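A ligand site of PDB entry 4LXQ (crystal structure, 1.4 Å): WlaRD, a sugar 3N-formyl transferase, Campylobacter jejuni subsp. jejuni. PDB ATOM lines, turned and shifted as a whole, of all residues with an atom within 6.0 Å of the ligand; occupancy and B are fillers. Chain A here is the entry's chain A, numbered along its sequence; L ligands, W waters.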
ATOM      1  N   LYS A  11     -26.483  -1.471 -12.799  1.00  0.00           N
ATOM      2  CA  LYS A  11     -27.841  -1.155 -12.318  1.00  0.00           C
ATOM      3  C   LYS A  11     -28.576  -0.210 -13.249  1.00  0.00           C
ATOM      4  O   LYS A  11     -28.009   0.432 -14.135  1.00  0.00           O
ATOM      5  CB  LYS A  11     -27.743  -0.525 -10.918  1.00  0.00           C
ATOM      6  CG  LYS A  11     -27.117   0.868 -10.871  1.00  0.00           C
ATOM      7  CD  LYS A  11     -27.360   1.525  -9.508  1.00  0.00           C
ATOM      8  CE  LYS A  11     -26.542   2.786  -9.396  1.00  0.00           C
ATOM      9  NZ  LYS A  11     -26.785   3.442  -8.033  1.00  0.00           N
ATOM     10  N   TRP A  46     -37.789   3.867  -8.880  1.00  0.00           N
ATOM     11  CA  TRP A  46     -37.748   4.932  -9.879  1.00  0.00           C
ATOM     12  C   TRP A  46     -36.789   4.585 -11.041  1.00  0.00           C
ATOM     13  O   TRP A  46     -36.737   5.291 -12.064  1.00  0.00           O
ATOM     14  CB  TRP A  46     -37.367   6.260  -9.212  1.00  0.00           C
ATOM     15  CG  TRP A  46     -36.068   6.234  -8.491  1.00  0.00           C
ATOM     16  CD1 TRP A  46     -35.821   5.807  -7.208  1.00  0.00           C
ATOM     17  CD2 TRP A  46     -34.804   6.696  -9.007  1.00  0.00           C
ATOM     18  NE1 TRP A  46     -34.477   5.956  -6.916  1.00  0.00           N
ATOM     19  CE2 TRP A  46     -33.844   6.521  -7.999  1.00  0.00           C
ATOM     20  CE3 TRP A  46     -34.425   7.256 -10.239  1.00  0.00           C
ATOM     21  CZ2 TRP A  46     -32.482   6.849  -8.204  1.00  0.00           C
ATOM     22  CZ3 TRP A  46     -33.088   7.610 -10.418  1.00  0.00           C
ATOM     23  CH2 TRP A  46     -32.143   7.379  -9.429  1.00  0.00           C
ATOM     24  N   GLU A  79     -22.963   1.299 -14.834  1.00  0.00           N
ATOM     25  CA  GLU A  79     -23.179   1.788 -13.469  1.00  0.00           C
ATOM     26  C   GLU A  79     -22.820   0.807 -12.384  1.00  0.00           C
ATOM     27  O   GLU A  79     -23.275   0.870 -11.247  1.00  0.00           O
ATOM     28  CB  GLU A  79     -24.604   2.368 -13.276  1.00  0.00           C
ATOM     29  CG  GLU A  79     -24.928   3.500 -14.267  1.00  0.00           C
ATOM     30  CD  GLU A  79     -23.870   4.583 -14.216  1.00  0.00           C
ATOM     31  OE1 GLU A  79     -23.836   5.310 -13.180  1.00  0.00           O
ATOM     32  OE2 GLU A  79     -23.027   4.716 -15.154  1.00  0.00           O
ATOM     33  N   PHE A  80     -21.867  -0.076 -12.701  1.00  0.00           N
ATOM     34  CA  PHE A  80     -21.378  -1.033 -11.700  1.00  0.00           C
ATOM     35  C   PHE A  80     -20.575  -0.368 -10.580  1.00  0.00           C
ATOM     36  O   PHE A  80     -19.910   0.664 -10.792  1.00  0.00           O
ATOM     37  CB  PHE A  80     -20.463  -2.058 -12.419  1.00  0.00           C
ATOM     38  CG  PHE A  80     -20.107  -3.289 -11.639  1.00  0.00           C
ATOM     39  CD1 PHE A  80     -18.802  -3.753 -11.728  1.00  0.00           C
ATOM     40  CD2 PHE A  80     -21.008  -4.000 -10.853  1.00  0.00           C
ATOM     41  CE1 PHE A  80     -18.392  -4.946 -11.088  1.00  0.00           C
ATOM     42  CE2 PHE A  80     -20.595  -5.183 -10.160  1.00  0.00           C
ATOM     43  CZ  PHE A  80     -19.298  -5.636 -10.288  1.00  0.00           C
ATOM     44  N   GLY A 107     -14.508   9.735 -11.812  1.00  0.00           N
ATOM     45  CA  GLY A 107     -14.894   9.535 -10.408  1.00  0.00           C
ATOM     46  C   GLY A 107     -16.411   9.480 -10.280  1.00  0.00           C
ATOM     47  O   GLY A 107     -17.093   8.873 -11.139  1.00  0.00           O
ATOM     48  N   VAL A 108     -16.930  10.091  -9.207  1.00  0.00           N
ATOM     49  CA  VAL A 108     -18.301   9.807  -8.818  1.00  0.00           C
ATOM     50  C   VAL A 108     -19.179  11.065  -8.822  1.00  0.00           C
ATOM     51  O   VAL A 108     -18.713  12.176  -9.104  1.00  0.00           O
ATOM     52  CB  VAL A 108     -18.325   9.193  -7.389  1.00  0.00           C
ATOM     53  CG1 VAL A 108     -17.564   7.843  -7.418  1.00  0.00           C
ATOM     54  CG2 VAL A 108     -17.699  10.111  -6.370  1.00  0.00           C
ATOM     55  N   PHE A 109     -20.460  10.822  -8.549  1.00  0.00           N
ATOM     56  CA  PHE A 109     -21.443  11.919  -8.422  1.00  0.00           C
ATOM     57  C   PHE A 109     -21.403  12.776  -9.685  1.00  0.00           C
ATOM     58  O   PHE A 109     -21.438  14.025  -9.618  1.00  0.00           O
ATOM     59  CB  PHE A 109     -21.200  12.773  -7.174  1.00  0.00           C
ATOM     60  CG  PHE A 109     -21.445  12.041  -5.886  1.00  0.00           C
ATOM     61  CD1 PHE A 109     -20.817  12.493  -4.732  1.00  0.00           C
ATOM     62  CD2 PHE A 109     -22.228  10.897  -5.846  1.00  0.00           C
ATOM     63  CE1 PHE A 109     -21.049  11.842  -3.514  1.00  0.00           C
ATOM     64  CE2 PHE A 109     -22.462  10.219  -4.642  1.00  0.00           C
ATOM     65  CZ  PHE A 109     -21.873  10.715  -3.484  1.00  0.00           C
ATOM     66  N   THR A 110     -21.373  12.168 -10.863  1.00  0.00           N
ATOM     67  CA  THR A 110     -21.198  12.929 -12.087  1.00  0.00           C
ATOM     68  C   THR A 110     -22.437  13.648 -12.618  1.00  0.00           C
ATOM     69  O   THR A 110     -22.357  14.336 -13.613  1.00  0.00           O
ATOM     70  CB  THR A 110     -20.585  12.078 -13.218  1.00  0.00           C
ATOM     71  OG1 THR A 110     -21.553  11.098 -13.599  1.00  0.00           O
ATOM     72  CG2 THR A 110     -19.259  11.422 -12.835  1.00  0.00           C
ATOM     73  N   SER A 111     -23.577  13.505 -11.934  1.00  0.00           N
ATOM     74  CA  SER A 111     -24.718  14.398 -12.198  1.00  0.00           C
ATOM     75  C   SER A 111     -24.602  15.668 -11.372  1.00  0.00           C
ATOM     76  O   SER A 111     -25.375  16.597 -11.647  1.00  0.00           O
ATOM     77  CB  SER A 111     -26.032  13.674 -11.877  1.00  0.00           C
ATOM     78  OG  SER A 111     -26.182  12.534 -12.705  1.00  0.00           O
ATOM     79  N   ILE A 112     -23.713  15.698 -10.408  1.00  0.00           N
ATOM     80  CA  ILE A 112     -23.486  16.870  -9.539  1.00  0.00           C
ATOM     81  C   ILE A 112     -22.287  17.645 -10.034  1.00  0.00           C
ATOM     82  O   ILE A 112     -22.340  18.886 -10.219  1.00  0.00           O
ATOM     83  CB  ILE A 112     -23.275  16.457  -8.083  1.00  0.00           C
ATOM     84  CG1 ILE A 112     -24.470  15.645  -7.584  1.00  0.00           C
ATOM     85  CG2 ILE A 112     -22.968  17.688  -7.206  1.00  0.00           C
ATOM     86  CD1 ILE A 112     -24.386  15.197  -6.152  1.00  0.00           C
ATOM     87  N   ALA A 152     -29.498  18.132 -11.106  1.00  0.00           N
ATOM     88  CA  ALA A 152     -28.729  16.896 -11.151  1.00  0.00           C
ATOM     89  C   ALA A 152     -29.616  15.735 -11.594  1.00  0.00           C
ATOM     90  O   ALA A 152     -29.166  14.866 -12.398  1.00  0.00           O
ATOM     91  CB  ALA A 152     -28.130  16.637  -9.774  1.00  0.00           C
ATOM     92  N   TYR A 156     -28.995  13.279 -14.748  1.00  0.00           N
ATOM     93  CA  TYR A 156     -28.912  11.825 -14.610  1.00  0.00           C
ATOM     94  C   TYR A 156     -29.830  11.115 -15.589  1.00  0.00           C
ATOM     95  O   TYR A 156     -29.434  10.113 -16.217  1.00  0.00           O
ATOM     96  CB  TYR A 156     -29.207  11.414 -13.175  1.00  0.00           C
ATOM     97  CG  TYR A 156     -28.929   9.943 -12.936  1.00  0.00           C
ATOM     98  CD1 TYR A 156     -27.608   9.479 -12.849  1.00  0.00           C
ATOM     99  CD2 TYR A 156     -29.970   9.027 -12.804  1.00  0.00           C
ATOM    100  CE1 TYR A 156     -27.321   8.122 -12.647  1.00  0.00           C
ATOM    101  CE2 TYR A 156     -29.683   7.683 -12.584  1.00  0.00           C
ATOM    102  CZ  TYR A 156     -28.379   7.252 -12.470  1.00  0.00           C
ATOM    103  OH  TYR A 156     -28.147   5.883 -12.285  1.00  0.00           O
ATOM    104  N   TYR A 159     -28.193  11.089 -18.842  1.00  0.00           N
ATOM    105  CA  TYR A 159     -27.125  10.078 -18.969  1.00  0.00           C
ATOM    106  C   TYR A 159     -27.753   8.718 -19.244  1.00  0.00           C
ATOM    107  O   TYR A 159     -27.225   7.942 -20.051  1.00  0.00           O
ATOM    108  CB  TYR A 159     -26.363   9.972 -17.654  1.00  0.00           C
ATOM    109  CG  TYR A 159     -25.438  11.128 -17.330  1.00  0.00           C
ATOM    110  CD1 TYR A 159     -24.627  11.738 -18.283  1.00  0.00           C
ATOM    111  CD2 TYR A 159     -25.307  11.558 -16.004  1.00  0.00           C
ATOM    112  CE1 TYR A 159     -23.751  12.751 -17.936  1.00  0.00           C
ATOM    113  CE2 TYR A 159     -24.423  12.577 -15.657  1.00  0.00           C
ATOM    114  CZ  TYR A 159     -23.648  13.138 -16.617  1.00  0.00           C
ATOM    115  OH  TYR A 159     -22.810  14.164 -16.290  1.00  0.00           O
ATOM    116  N   ARG A 194     -15.830  10.707  -3.518  1.00  0.00           N
ATOM    117  CA  ARG A 194     -16.933  10.946  -2.597  1.00  0.00           C
ATOM    118  C   ARG A 194     -16.567  11.929  -1.507  1.00  0.00           C
ATOM    119  O   ARG A 194     -17.397  12.760  -1.159  1.00  0.00           O
ATOM    120  CB  ARG A 194     -17.450   9.629  -1.990  1.00  0.00           C
ATOM    121  CG  ARG A 194     -18.252   8.849  -3.000  1.00  0.00           C
ATOM    122  CD  ARG A 194     -19.024   7.616  -2.496  1.00  0.00           C
ATOM    123  NE  ARG A 194     -19.357   6.815  -3.684  1.00  0.00           N
ATOM    124  CZ  ARG A 194     -18.651   5.766  -4.113  1.00  0.00           C
ATOM    125  NH1 ARG A 194     -17.591   5.334  -3.436  1.00  0.00           N
ATOM    126  NH2 ARG A 194     -19.024   5.127  -5.228  1.00  0.00           N
ATOM    127  N   LEU A 199     -22.671  16.361   0.370  1.00  0.00           N
ATOM    128  CA  LEU A 199     -24.033  16.323  -0.149  1.00  0.00           C
ATOM    129  C   LEU A 199     -24.998  17.239   0.580  1.00  0.00           C
ATOM    130  O   LEU A 199     -26.117  17.468   0.090  1.00  0.00           O
ATOM    131  CB  LEU A 199     -24.582  14.897  -0.100  1.00  0.00           C
ATOM    132  CG  LEU A 199     -23.873  13.989  -1.108  1.00  0.00           C
ATOM    133  CD1 LEU A 199     -24.208  12.530  -0.786  1.00  0.00           C
ATOM    134  CD2 LEU A 199     -24.291  14.394  -2.537  1.00  0.00           C
ATOM    135  N   ALA A 218     -27.298  21.682  -8.620  1.00  0.00           N
ATOM    136  CA  ALA A 218     -26.392  20.531  -8.644  1.00  0.00           C
ATOM    137  C   ALA A 218     -26.776  19.517  -7.578  1.00  0.00           C
ATOM    138  O   ALA A 218     -26.403  18.326  -7.696  1.00  0.00           O
ATOM    139  CB  ALA A 218     -24.985  20.977  -8.425  1.00  0.00           C
ATOM    140  N   PHE A 219     -27.518  19.914  -6.545  1.00  0.00           N
ATOM    141  CA  PHE A 219     -27.886  19.017  -5.458  1.00  0.00           C
ATOM    142  C   PHE A 219     -29.350  18.637  -5.463  1.00  0.00           C
ATOM    143  O   PHE A 219     -29.781  17.913  -4.541  1.00  0.00           O
ATOM    144  CB  PHE A 219     -27.434  19.533  -4.077  1.00  0.00           C
ATOM    145  CG  PHE A 219     -25.939  19.627  -3.946  1.00  0.00           C
ATOM    146  CD1 PHE A 219     -25.220  18.522  -3.538  1.00  0.00           C
ATOM    147  CD2 PHE A 219     -25.213  20.755  -4.373  1.00  0.00           C
ATOM    148  CE1 PHE A 219     -23.837  18.565  -3.452  1.00  0.00           C
ATOM    149  CE2 PHE A 219     -23.822  20.804  -4.287  1.00  0.00           C
ATOM    150  CZ  PHE A 219     -23.132  19.699  -3.822  1.00  0.00           C
ATOM    151  N   PHE A 221     -31.862  16.336  -6.319  1.00  0.00           N
ATOM    152  CA  PHE A 221     -32.089  14.974  -6.837  1.00  0.00           C
ATOM    153  C   PHE A 221     -32.901  14.264  -5.747  1.00  0.00           C
ATOM    154  O   PHE A 221     -32.322  13.622  -4.848  1.00  0.00           O
ATOM    155  CB  PHE A 221     -30.742  14.264  -7.125  1.00  0.00           C
ATOM    156  CG  PHE A 221     -30.835  13.048  -8.029  1.00  0.00           C
ATOM    157  CD1 PHE A 221     -29.794  12.785  -8.908  1.00  0.00           C
ATOM    158  CD2 PHE A 221     -31.908  12.174  -7.992  1.00  0.00           C
ATOM    159  CE1 PHE A 221     -29.830  11.638  -9.737  1.00  0.00           C
ATOM    160  CE2 PHE A 221     -31.957  11.057  -8.825  1.00  0.00           C
ATOM    161  CZ  PHE A 221     -30.887  10.773  -9.663  1.00  0.00           C
ATOM    162  N   TYR A 224     -32.550  11.236  -3.398  1.00  0.00           N
ATOM    163  CA  TYR A 224     -31.433  11.298  -2.473  1.00  0.00           C
ATOM    164  C   TYR A 224     -31.488  12.463  -1.482  1.00  0.00           C
ATOM    165  O   TYR A 224     -31.496  12.270  -0.255  1.00  0.00           O
ATOM    166  CB  TYR A 224     -30.136  11.362  -3.294  1.00  0.00           C
ATOM    167  CG  TYR A 224     -29.899  10.115  -4.131  1.00  0.00           C
ATOM    168  CD1 TYR A 224     -29.463   8.926  -3.518  1.00  0.00           C
ATOM    169  CD2 TYR A 224     -30.108  10.126  -5.510  1.00  0.00           C
ATOM    170  CE1 TYR A 224     -29.232   7.788  -4.295  1.00  0.00           C
ATOM    171  CE2 TYR A 224     -29.873   8.969  -6.278  1.00  0.00           C
ATOM    172  CZ  TYR A 224     -29.416   7.846  -5.658  1.00  0.00           C
ATOM    173  OH  TYR A 224     -29.217   6.715  -6.449  1.00  0.00           O
ATOM    174  N   GLN A 225     -31.522  13.691  -2.015  1.00  0.00           N
ATOM    175  CA  GLN A 225     -31.584  14.872  -1.145  1.00  0.00           C
ATOM    176  C   GLN A 225     -32.060  16.045  -1.972  1.00  0.00           C
ATOM    177  O   GLN A 225     -32.092  16.042  -3.200  1.00  0.00           O
ATOM    178  CB  GLN A 225     -30.247  15.187  -0.488  1.00  0.00           C
ATOM    179  CG  GLN A 225     -29.178  15.822  -1.421  1.00  0.00           C
ATOM    180  CD  GLN A 225     -28.579  14.842  -2.444  1.00  0.00           C
ATOM    181  OE1 GLN A 225     -28.063  13.760  -2.075  1.00  0.00           O
ATOM    182  NE2 GLN A 225     -28.661  15.187  -3.726  1.00  0.00           N
HETATM  183  P1  LIG L   1     -24.665   6.639  -7.997  1.00  0.00           P
HETATM  184  O1  LIG L   1     -24.293   6.031  -9.340  1.00  0.00           O
HETATM  185  O2  LIG L   1     -25.643   5.875  -7.130  1.00  0.00           O
HETATM  186  O3  LIG L   1     -23.346   6.854  -7.119  1.00  0.00           O
HETATM  187  P2  LIG L   1     -21.778   6.935  -7.598  1.00  0.00           P
HETATM  188  O4  LIG L   1     -21.570   8.247  -8.308  1.00  0.00           O
HETATM  189  O5  LIG L   1     -21.474   5.636  -8.334  1.00  0.00           O
HETATM  190  O6  LIG L   1     -21.113   6.847  -6.246  1.00  0.00           O
HETATM  191  O7  LIG L   1     -25.205   8.114  -8.145  1.00  0.00           O
HETATM  192  C1  LIG L   1     -25.978   8.493  -9.280  1.00  0.00           C
HETATM  193  C2  LIG L   1     -26.323   9.971  -9.164  1.00  0.00           C
HETATM  194  O8  LIG L   1     -27.255  10.048  -8.042  1.00  0.00           O
HETATM  195  C3  LIG L   1     -25.163  10.882  -8.732  1.00  0.00           C
HETATM  196  O9  LIG L   1     -24.488  11.388  -9.889  1.00  0.00           O
HETATM  197  C4  LIG L   1     -25.943  12.031  -8.085  1.00  0.00           C
HETATM  198  C5  LIG L   1     -27.050  11.287  -7.375  1.00  0.00           C
HETATM  199  N1  LIG L   1     -26.792  11.051  -5.954  1.00  0.00           N
HETATM  200  C6  LIG L   1     -27.134  12.004  -5.073  1.00  0.00           C
HETATM  201  O10 LIG L   1     -27.583  13.120  -5.474  1.00  0.00           O
HETATM  202  N2  LIG L   1     -26.951  11.784  -3.753  1.00  0.00           N
HETATM  203  C7  LIG L   1     -26.515  10.587  -3.260  1.00  0.00           C
HETATM  204  O11 LIG L   1     -26.476  10.430  -2.017  1.00  0.00           O
HETATM  205  C8  LIG L   1     -26.141   9.584  -4.168  1.00  0.00           C
HETATM  206  C9  LIG L   1     -25.650   8.233  -3.666  1.00  0.00           C
HETATM  207  C10 LIG L   1     -26.351   9.852  -5.514  1.00  0.00           C
HETATM  208  O   HOH W   1     -20.078   7.269 -10.721  1.00  0.00           O
HETATM  209  O   HOH W   2     -25.805   5.256 -11.486  1.00  0.00           O
HETATM  210  O   HOH W   3     -24.982   8.921  -0.340  1.00  0.00           O
HETATM  211  O   HOH W   4     -22.642   9.470 -10.389  1.00  0.00           O
HETATM  212  O   HOH W   5     -24.279  10.440 -12.906  1.00  0.00           O
HETATM  213  O   HOH W   6     -24.886   4.729  -4.913  1.00  0.00           O
HETATM  214  O   HOH W   7     -22.511   6.145  -3.914  1.00  0.00           O
HETATM  215  O   HOH W   8     -22.898   2.949  -9.263  1.00  0.00           O
HETATM  216  O   HOH W   9     -21.900   4.915 -11.423  1.00  0.00           O
HETATM  217  O   HOH W  10     -19.177   4.538  -8.375  1.00  0.00           O
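Residues that only touch the ligand: Glu 79, Val 108, Ile 112, Tyr 156, Leu 199, Phe 221 and Tyr 224.
Hydrophobic or aromatic side chains that line the ligand: Val 108, Phe 109, Ile 112, Tyr 156, Leu 199, Phe 221 and Tyr 224.
The backbone carbonyl oxygen (O) of Thr 110 sits at hydrogen-bond distance from the side-chain hydroxyl (OH) of Tyr 159, 2.7 Å away.
NE2 of Gln 225 sits at hydrogen-bond distance from O of Phe 219 (3.1 Å).
Water W10 lies within hydrogen-bond range of an oxygen (O5) of the ligand (2.5 Å) and the guanidinium group (NH2) of Arg 194 (3.2 Å).
Water W4 lies within hydrogen-bond range of O4 of the ligand (2.6 Å), N of Thr 110 (3.0 Å) and N of Phe 109 (3.2 Å).
Water W2 lies within hydrogen-bond range of OH of Tyr 156, OE1 of Glu 79 and O1 of the ligand.
Water W1 bridges O4 of the ligand (3.0 Å) and O of Gly 107 (3.4 Å).
Water W5 lies within hydrogen-bond range of OG of Ser 111, OG1 of Thr 110 and O9 of the ligand.
Water W8 bridges the backbone carbonyl oxygen (O) of Glu 79 and an oxygen (O5) of the ligand.
N of Ser 111 is in hydrogen-bond range of O9 of the ligand (3.1 Å).
O6 of the ligand is in salt-bridge range of NH2 of Arg 194, at 2.9 Å.
An oxygen (O9) of the ligand sits at hydrogen-bond distance from the backbone NH (N) of Thr 110, 3.4 Å away.
A nitrogen (N2) of the ligand sits at hydrogen-bond distance from the side-chain amide oxygen (OE1) of Gln 225, at 2.8 Å.
The side-chain amino group (NZ) of Lys 11 lies within salt-bridge range of an oxygen (O2) of the ligand (2.8 Å).
An oxygen (O9) of the ligand sits close to the side-chain hydroxyl (OG) of Ser 111 (3.5 Å).
An oxygen (O4) of the ligand lies within hydrogen-bond range of the backbone NH (N) of Phe 109 (2.8 Å).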
